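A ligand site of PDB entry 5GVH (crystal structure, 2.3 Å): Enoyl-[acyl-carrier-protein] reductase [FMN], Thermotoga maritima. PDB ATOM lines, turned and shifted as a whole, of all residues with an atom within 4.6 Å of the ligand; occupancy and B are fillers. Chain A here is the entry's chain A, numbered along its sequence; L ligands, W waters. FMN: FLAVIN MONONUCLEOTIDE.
N of Thr 194 lies within hydrogen-bond range of O3P of the ligand (3.1 Å). O3P of the ligand sits at hydrogen-bond distance from OG1 of Thr 194. The side-chain carboxylate (OE2) of Glu 139 lies within hydrogen-bond range of an oxygen (O3') of the ligand. The side-chain amide nitrogen of Gln 191 sits at hydrogen-bond distance from an oxygen (O3') of the ligand (2.7 Å). An oxygen (O1P) of the ligand lies within hydrogen-bond range of the side-chain hydroxyl (OG) of Ser 280 (2.8 Å). O2' of the ligand is in hydrogen-bond range of N of Gly 21 (3.5 Å). The backbone carbonyl oxygen (O) of Gly 21 lies close to an oxygen (O2') of the ligand (2.9 Å). The backbone NH of Gly 193 is in hydrogen-bond range of an oxygen (O2P) of the ligand, 2.9 Å away. N of Gly 172 lies within hydrogen-bond range of O1P of the ligand (2.9 Å). The side-chain amide nitrogen (ND2) of Asn 71 sits close to a nitrogen (N3) of the ligand. N of Ala 23 lies within hydrogen-bond range of N5 of the ligand (3.2 Å).
The backbone NH of Gly 278 lies within hydrogen-bond range of the side-chain hydroxyl of Thr 194, 3.1 Å away. The side-chain carboxylate of Glu 139 lies within hydrogen-bond range of the side-chain hydroxyl of Ser 143 (3.0 Å). The backbone carbonyl oxygen of Met 276 is in hydrogen-bond range of the side-chain hydroxyl of Tyr 208 (2.8 Å). The backbone NH (N) of Gly 20 sits at hydrogen-bond distance from the backbone carbonyl oxygen (O) of Met 192.
Merely in contact with the ligand: Gly 20 (3.3 Å), Met 22 (3.2 Å), Ile 73 (3.2 Å), Gly 97 (3.3 Å), Ser 143 (3.1 Å), Gly 144 (3.4 Å), Gly 171 (3.5 Å), Met 192 (3.6 Å), Tyr 208 (3.4 Å), Met 276 (3.1 Å) and Gly 278 (3.8 Å). Hydrophobic or aromatic side chains within 4 Å of the ligand: Met 22, Ala 23, Ile 73 and Met 276. 20 residues have an atom within 4 Å of the ligand: Gly 20, Gly 21, Met 22, Ala 23, Asn 71, Ile 73, Gly 97, Glu 139, Ser 143, Gly 144, Gly 171, Gly 172, Gln 191, Met 192, Gly 193, Thr 194, Tyr 208, Met 276, Gly 278 and Ser 280. The nearest printed residue that does not touch the ligand is Ile 173 (4.03 Å).
Water W1 lies within hydrogen-bond range of an oxygen (O2P) of the ligand (2.6 Å), the backbone carbonyl oxygen of Ile 173 (3.0 Å), the side-chain hydroxyl of Ser 280 (3.3 Å) and the backbone NH of Thr 194 (3.5 Å).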
ATOM      1  N   GLY A  20      30.465  23.138 -17.429  1.00  0.00           N
ATOM      2  CA  GLY A  20      30.666  24.532 -17.094  1.00  0.00           C
ATOM      3  C   GLY A  20      31.776  24.755 -16.074  1.00  0.00           C
ATOM      4  O   GLY A  20      31.844  24.067 -15.055  1.00  0.00           O
ATOM      5  N   GLY A  21      32.670  25.715 -16.346  1.00  0.00           N
ATOM      6  CA  GLY A  21      33.655  26.084 -15.356  1.00  0.00           C
ATOM      7  C   GLY A  21      32.968  26.548 -14.090  1.00  0.00           C
ATOM      8  O   GLY A  21      32.058  27.374 -14.182  1.00  0.00           O
ATOM      9  N   MET A  22      33.351  26.021 -12.924  1.00  0.00           N
ATOM     10  CA  MET A  22      32.649  26.330 -11.674  1.00  0.00           C
ATOM     11  C   MET A  22      33.659  26.533 -10.548  1.00  0.00           C
ATOM     12  O   MET A  22      34.469  25.657 -10.266  1.00  0.00           O
ATOM     13  CB  MET A  22      31.654  25.205 -11.295  1.00  0.00           C
ATOM     14  CG  MET A  22      30.429  25.048 -12.225  1.00  0.00           C
ATOM     15  SD  MET A  22      29.267  23.722 -11.743  1.00  0.00           S
ATOM     16  CE  MET A  22      30.175  22.264 -12.307  1.00  0.00           C
ATOM     17  N   ALA A  23      33.602  27.699  -9.902  1.00  0.00           N
ATOM     18  CA  ALA A  23      34.482  27.953  -8.769  1.00  0.00           C
ATOM     19  C   ALA A  23      34.183  27.170  -7.496  1.00  0.00           C
ATOM     20  O   ALA A  23      33.084  27.274  -6.940  1.00  0.00           O
ATOM     21  CB  ALA A  23      34.385  29.406  -8.321  1.00  0.00           C
ATOM     22  N   ASN A  71      38.658  27.325 -16.737  1.00  0.00           N
ATOM     23  CA  ASN A  71      37.808  28.509 -16.676  1.00  0.00           C
ATOM     24  C   ASN A  71      38.444  29.582 -15.803  1.00  0.00           C
ATOM     25  O   ASN A  71      38.785  29.304 -14.645  1.00  0.00           O
ATOM     26  CB  ASN A  71      36.417  28.165 -16.138  1.00  0.00           C
ATOM     27  CG  ASN A  71      35.558  29.414 -15.888  1.00  0.00           C
ATOM     28  OD1 ASN A  71      35.016  29.989 -16.832  1.00  0.00           O
ATOM     29  ND2 ASN A  71      35.449  29.843 -14.636  1.00  0.00           N
ATOM     30  N   ILE A  73      38.008  33.578 -14.227  1.00  0.00           N
ATOM     31  CA  ILE A  73      37.187  34.756 -13.949  1.00  0.00           C
ATOM     32  C   ILE A  73      38.022  36.017 -14.194  1.00  0.00           C
ATOM     33  O   ILE A  73      39.018  36.261 -13.503  1.00  0.00           O
ATOM     34  CB  ILE A  73      36.659  34.744 -12.510  1.00  0.00           C
ATOM     35  CG1 ILE A  73      36.175  33.365 -12.123  1.00  0.00           C
ATOM     36  CG2 ILE A  73      35.466  35.696 -12.385  1.00  0.00           C
ATOM     37  CD1 ILE A  73      35.039  32.903 -12.976  1.00  0.00           C
ATOM     38  N   PHE A  96      36.354  31.679 -20.395  1.00  0.00           N
ATOM     39  CA  PHE A  96      36.343  32.914 -19.619  1.00  0.00           C
ATOM     40  C   PHE A  96      34.963  33.189 -19.061  1.00  0.00           C
ATOM     41  O   PHE A  96      33.948  32.998 -19.748  1.00  0.00           O
ATOM     42  CB  PHE A  96      36.831  34.087 -20.463  1.00  0.00           C
ATOM     43  CG  PHE A  96      38.315  34.128 -20.618  1.00  0.00           C
ATOM     44  CD1 PHE A  96      38.915  33.856 -21.833  1.00  0.00           C
ATOM     45  CD2 PHE A  96      39.126  34.428 -19.530  1.00  0.00           C
ATOM     46  CE1 PHE A  96      40.311  33.886 -21.963  1.00  0.00           C
ATOM     47  CE2 PHE A  96      40.513  34.462 -19.649  1.00  0.00           C
ATOM     48  CZ  PHE A  96      41.099  34.193 -20.867  1.00  0.00           C
ATOM     49  N   GLY A  97      34.921  33.619 -17.811  1.00  0.00           N
ATOM     50  CA  GLY A  97      33.675  33.997 -17.187  1.00  0.00           C
ATOM     51  C   GLY A  97      33.135  35.303 -17.730  1.00  0.00           C
ATOM     52  O   GLY A  97      33.559  35.763 -18.795  1.00  0.00           O
ATOM     53  N   GLU A 139      25.080  31.964 -22.557  1.00  0.00           N
ATOM     54  CA  GLU A 139      24.542  31.509 -21.285  1.00  0.00           C
ATOM     55  C   GLU A 139      23.307  32.323 -20.909  1.00  0.00           C
ATOM     56  O   GLU A 139      23.399  33.515 -20.613  1.00  0.00           O
ATOM     57  CB  GLU A 139      25.581  31.618 -20.179  1.00  0.00           C
ATOM     58  CG  GLU A 139      25.065  31.005 -18.889  1.00  0.00           C
ATOM     59  CD  GLU A 139      25.855  31.394 -17.678  1.00  0.00           C
ATOM     60  OE1 GLU A 139      25.659  32.530 -17.183  1.00  0.00           O
ATOM     61  OE2 GLU A 139      26.647  30.565 -17.189  1.00  0.00           O
ATOM     62  N   GLU A 142      18.652  31.725 -16.804  1.00  0.00           N
ATOM     63  CA  GLU A 142      18.249  30.632 -15.928  1.00  0.00           C
ATOM     64  C   GLU A 142      19.422  29.816 -15.413  1.00  0.00           C
ATOM     65  O   GLU A 142      19.220  28.891 -14.620  1.00  0.00           O
ATOM     66  CB  GLU A 142      17.248  29.696 -16.637  1.00  0.00           C
ATOM     67  CG  GLU A 142      17.706  29.157 -17.980  1.00  0.00           C
ATOM     68  CD  GLU A 142      17.374  30.114 -19.122  1.00  0.00           C
ATOM     69  OE1 GLU A 142      17.968  31.221 -19.141  1.00  0.00           O
ATOM     70  OE2 GLU A 142      16.505  29.775 -19.959  1.00  0.00           O
ATOM     71  N   SER A 143      20.643  30.143 -15.820  1.00  0.00           N
ATOM     72  CA  SER A 143      21.791  29.361 -15.395  1.00  0.00           C
ATOM     73  C   SER A 143      22.126  29.624 -13.927  1.00  0.00           C
ATOM     74  O   SER A 143      21.655  30.593 -13.306  1.00  0.00           O
ATOM     75  CB  SER A 143      23.006  29.674 -16.267  1.00  0.00           C
ATOM     76  OG  SER A 143      23.374  31.024 -16.074  1.00  0.00           O
ATOM     77  N   GLY A 144      22.958  28.736 -13.365  1.00  0.00           N
ATOM     78  CA  GLY A 144      23.495  28.975 -12.045  1.00  0.00           C
ATOM     79  C   GLY A 144      24.715  29.854 -12.085  1.00  0.00           C
ATOM     80  O   GLY A 144      25.384  29.984 -13.107  1.00  0.00           O
ATOM     81  N   GLY A 145      25.006  30.470 -10.938  1.00  0.00           N
ATOM     82  CA  GLY A 145      26.094  31.431 -10.888  1.00  0.00           C
ATOM     83  C   GLY A 145      25.673  32.767 -11.476  1.00  0.00           C
ATOM     84  O   GLY A 145      24.467  33.064 -11.617  1.00  0.00           O
ATOM     85  N   ALA A 170      24.208  27.346 -22.984  1.00  0.00           N
ATOM     86  CA  ALA A 170      24.351  27.092 -21.550  1.00  0.00           C
ATOM     87  C   ALA A 170      23.194  27.709 -20.785  1.00  0.00           C
ATOM     88  O   ALA A 170      22.678  28.771 -21.156  1.00  0.00           O
ATOM     89  CB  ALA A 170      25.677  27.629 -21.012  1.00  0.00           C
ATOM     90  N   GLY A 171      22.811  27.059 -19.686  1.00  0.00           N
ATOM     91  CA  GLY A 171      21.747  27.592 -18.851  1.00  0.00           C
ATOM     92  C   GLY A 171      20.411  26.910 -19.090  1.00  0.00           C
ATOM     93  O   GLY A 171      19.732  27.124 -20.098  1.00  0.00           O
ATOM     94  N   GLY A 172      20.015  26.062 -18.133  1.00  0.00           N
ATOM     95  CA  GLY A 172      18.779  25.336 -18.217  1.00  0.00           C
ATOM     96  C   GLY A 172      18.847  23.997 -18.918  1.00  0.00           C
ATOM     97  O   GLY A 172      17.790  23.355 -19.073  1.00  0.00           O
ATOM     98  N   ILE A 173      20.033  23.546 -19.357  1.00  0.00           N
ATOM     99  CA  ILE A 173      20.150  22.262 -20.056  1.00  0.00           C
ATOM    100  C   ILE A 173      20.471  21.168 -19.046  1.00  0.00           C
ATOM    101  O   ILE A 173      21.494  21.240 -18.339  1.00  0.00           O
ATOM    102  CB  ILE A 173      21.215  22.305 -21.166  1.00  0.00           C
ATOM    103  CG1 ILE A 173      20.830  23.257 -22.303  1.00  0.00           C
ATOM    104  CG2 ILE A 173      21.341  20.928 -21.787  1.00  0.00           C
ATOM    105  CD1 ILE A 173      21.400  24.640 -22.201  1.00  0.00           C
ATOM    106  N   GLN A 191      26.557  23.201 -22.659  1.00  0.00           N
ATOM    107  CA  GLN A 191      27.341  23.271 -21.427  1.00  0.00           C
ATOM    108  C   GLN A 191      26.404  23.184 -20.233  1.00  0.00           C
ATOM    109  O   GLN A 191      25.389  23.895 -20.182  1.00  0.00           O
ATOM    110  CB  GLN A 191      28.162  24.559 -21.390  1.00  0.00           C
ATOM    111  CG  GLN A 191      28.662  24.938 -19.996  1.00  0.00           C
ATOM    112  CD  GLN A 191      29.555  26.179 -19.997  1.00  0.00           C
ATOM    113  OE1 GLN A 191      30.692  26.134 -20.457  1.00  0.00           O
ATOM    114  NE2 GLN A 191      29.052  27.301 -19.456  1.00  0.00           N
ATOM    115  N   MET A 192      26.728  22.321 -19.283  1.00  0.00           N
ATOM    116  CA  MET A 192      25.923  22.080 -18.106  1.00  0.00           C
ATOM    117  C   MET A 192      26.758  22.309 -16.849  1.00  0.00           C
ATOM    118  O   MET A 192      27.951  22.009 -16.832  1.00  0.00           O
ATOM    119  CB  MET A 192      25.340  20.646 -18.086  1.00  0.00           C
ATOM    120  CG  MET A 192      24.235  20.409 -19.108  1.00  0.00           C
ATOM    121  SD  MET A 192      23.610  18.710 -19.163  1.00  0.00           S
ATOM    122  CE  MET A 192      24.555  18.107 -20.546  1.00  0.00           C
ATOM    123  N   GLY A 193      26.130  22.855 -15.821  1.00  0.00           N
ATOM    124  CA  GLY A 193      26.793  22.991 -14.541  1.00  0.00           C
ATOM    125  C   GLY A 193      26.058  22.225 -13.464  1.00  0.00           C
ATOM    126  O   GLY A 193      26.601  21.264 -12.898  1.00  0.00           O
ATOM    127  N   THR A 194      24.806  22.626 -13.186  1.00  0.00           N
ATOM    128  CA  THR A 194      24.023  22.009 -12.116  1.00  0.00           C
ATOM    129  C   THR A 194      23.845  20.518 -12.340  1.00  0.00           C
ATOM    130  O   THR A 194      23.913  19.730 -11.390  1.00  0.00           O
ATOM    131  CB  THR A 194      22.648  22.700 -11.984  1.00  0.00           C
ATOM    132  OG1 THR A 194      22.817  24.124 -11.820  1.00  0.00           O
ATOM    133  CG2 THR A 194      21.869  22.164 -10.768  1.00  0.00           C
ATOM    134  N   TYR A 208      24.612  19.757  -0.710  1.00  0.00           N
ATOM    135  CA  TYR A 208      24.513  20.482  -1.976  1.00  0.00           C
ATOM    136  C   TYR A 208      23.844  19.645  -3.054  1.00  0.00           C
ATOM    137  O   TYR A 208      22.910  20.105  -3.712  1.00  0.00           O
ATOM    138  CB  TYR A 208      25.905  20.903  -2.436  1.00  0.00           C
ATOM    139  CG  TYR A 208      25.979  22.161  -3.262  1.00  0.00           C
ATOM    140  CD1 TYR A 208      25.219  22.336  -4.427  1.00  0.00           C
ATOM    141  CD2 TYR A 208      26.869  23.180  -2.902  1.00  0.00           C
ATOM    142  CE1 TYR A 208      25.316  23.491  -5.179  1.00  0.00           C
ATOM    143  CE2 TYR A 208      26.970  24.330  -3.648  1.00  0.00           C
ATOM    144  CZ  TYR A 208      26.207  24.486  -4.780  1.00  0.00           C
ATOM    145  OH  TYR A 208      26.336  25.651  -5.499  1.00  0.00           O
ATOM    146  N   LEU A 261      30.348  31.079  -1.249  1.00  0.00           N
ATOM    147  CA  LEU A 261      30.229  29.911  -2.117  1.00  0.00           C
ATOM    148  C   LEU A 261      30.934  28.712  -1.513  1.00  0.00           C
ATOM    149  O   LEU A 261      30.438  27.575  -1.649  1.00  0.00           O
ATOM    150  CB  LEU A 261      30.789  30.223  -3.503  1.00  0.00           C
ATOM    151  CG  LEU A 261      30.820  29.106  -4.550  1.00  0.00           C
ATOM    152  CD1 LEU A 261      29.439  28.487  -4.753  1.00  0.00           C
ATOM    153  CD2 LEU A 261      31.355  29.659  -5.850  1.00  0.00           C
ATOM    154  N   MET A 276      24.864  28.265  -5.513  1.00  0.00           N
ATOM    155  CA  MET A 276      24.662  28.624  -6.908  1.00  0.00           C
ATOM    156  C   MET A 276      24.108  27.428  -7.660  1.00  0.00           C
ATOM    157  O   MET A 276      24.712  26.350  -7.668  1.00  0.00           O
ATOM    158  CB  MET A 276      25.970  29.111  -7.545  1.00  0.00           C
ATOM    159  CG  MET A 276      26.409  30.496  -7.079  1.00  0.00           C
ATOM    160  SD  MET A 276      27.926  31.002  -7.892  1.00  0.00           S
ATOM    161  CE  MET A 276      28.109  32.668  -7.250  1.00  0.00           C
ATOM    162  N   VAL A 277      22.923  27.606  -8.247  1.00  0.00           N
ATOM    163  CA  VAL A 277      22.222  26.593  -9.023  1.00  0.00           C
ATOM    164  C   VAL A 277      21.378  27.309 -10.076  1.00  0.00           C
ATOM    165  O   VAL A 277      20.923  28.427  -9.884  1.00  0.00           O
ATOM    166  CB  VAL A 277      21.295  25.692  -8.163  1.00  0.00           C
ATOM    167  CG1 VAL A 277      22.088  24.696  -7.339  1.00  0.00           C
ATOM    168  CG2 VAL A 277      20.415  26.549  -7.271  1.00  0.00           C
ATOM    169  N   GLY A 278      21.187  26.630 -11.203  1.00  0.00           N
ATOM    170  CA  GLY A 278      20.265  27.104 -12.198  1.00  0.00           C
ATOM    171  C   GLY A 278      18.865  26.561 -11.969  1.00  0.00           C
ATOM    172  O   GLY A 278      18.662  25.663 -11.147  1.00  0.00           O
ATOM    173  N   SER A 280      17.497  24.708 -13.877  1.00  0.00           N
ATOM    174  CA  SER A 280      17.568  23.301 -14.258  1.00  0.00           C
ATOM    175  C   SER A 280      17.530  22.353 -13.064  1.00  0.00           C
ATOM    176  O   SER A 280      17.284  21.159 -13.258  1.00  0.00           O
ATOM    177  CB  SER A 280      18.851  23.031 -15.060  1.00  0.00           C
ATOM    178  OG  SER A 280      20.005  23.443 -14.354  1.00  0.00           O
HETATM  179  N1  FMN L   1      30.653  30.146 -14.689  1.00  0.00           N
HETATM  180  C2  FMN L   1      31.851  30.831 -14.860  1.00  0.00           C
HETATM  181  O2  FMN L   1      32.138  31.377 -15.925  1.00  0.00           O
HETATM  182  N3  FMN L   1      32.736  30.920 -13.817  1.00  0.00           N
HETATM  183  C4  FMN L   1      32.454  30.327 -12.607  1.00  0.00           C
HETATM  184  O4  FMN L   1      33.267  30.438 -11.698  1.00  0.00           O
HETATM  185  C4A FMN L   1      31.261  29.636 -12.430  1.00  0.00           C
HETATM  186  N5  FMN L   1      30.979  29.051 -11.214  1.00  0.00           N
HETATM  187  C5A FMN L   1      29.812  28.346 -11.038  1.00  0.00           C
HETATM  188  C6  FMN L   1      29.554  27.739  -9.814  1.00  0.00           C
HETATM  189  C7  FMN L   1      28.388  27.032  -9.608  1.00  0.00           C
HETATM  190  C7M FMN L   1      28.124  26.400  -8.275  1.00  0.00           C
HETATM  191  C8  FMN L   1      27.455  26.919 -10.654  1.00  0.00           C
HETATM  192  C8M FMN L   1      26.179  26.158 -10.435  1.00  0.00           C
HETATM  193  C9  FMN L   1      27.704  27.516 -11.883  1.00  0.00           C
HETATM  194  C9A FMN L   1      28.887  28.236 -12.088  1.00  0.00           C
HETATM  195  N10 FMN L   1      29.169  28.844 -13.313  1.00  0.00           N
HETATM  196  C10 FMN L   1      30.348  29.546 -13.486  1.00  0.00           C
HETATM  197  C1' FMN L   1      28.192  28.722 -14.449  1.00  0.00           C
HETATM  198  C2' FMN L   1      28.429  27.407 -15.190  1.00  0.00           C
HETATM  199  O2' FMN L   1      29.688  27.456 -15.829  1.00  0.00           O
HETATM  200  C3' FMN L   1      27.381  27.143 -16.268  1.00  0.00           C
HETATM  201  O3' FMN L   1      27.576  28.069 -17.315  1.00  0.00           O
HETATM  202  C4' FMN L   1      25.964  27.203 -15.722  1.00  0.00           C
HETATM  203  O4' FMN L   1      25.895  26.354 -14.598  1.00  0.00           O
HETATM  204  C5' FMN L   1      24.941  26.679 -16.726  1.00  0.00           C
HETATM  205  O5' FMN L   1      23.663  26.634 -16.133  1.00  0.00           O
HETATM  206  P   FMN L   1      22.988  25.284 -15.535  1.00  0.00           P
HETATM  207  O1P FMN L   1      21.487  25.401 -15.677  1.00  0.00           O
HETATM  208  O2P FMN L   1      23.484  24.044 -16.240  1.00  0.00           O
HETATM  209  O3P FMN L   1      23.294  25.213 -14.059  1.00  0.00           O
HETATM  210  O   HOH W   1      22.516  21.731 -15.612  1.00  0.00           O
HETATM  211  O   HOH W   2      29.671  32.978 -16.796  1.00  0.00           O
HETATM  212  O   HOH W   3      22.917  24.306 -18.929  1.00  0.00           O
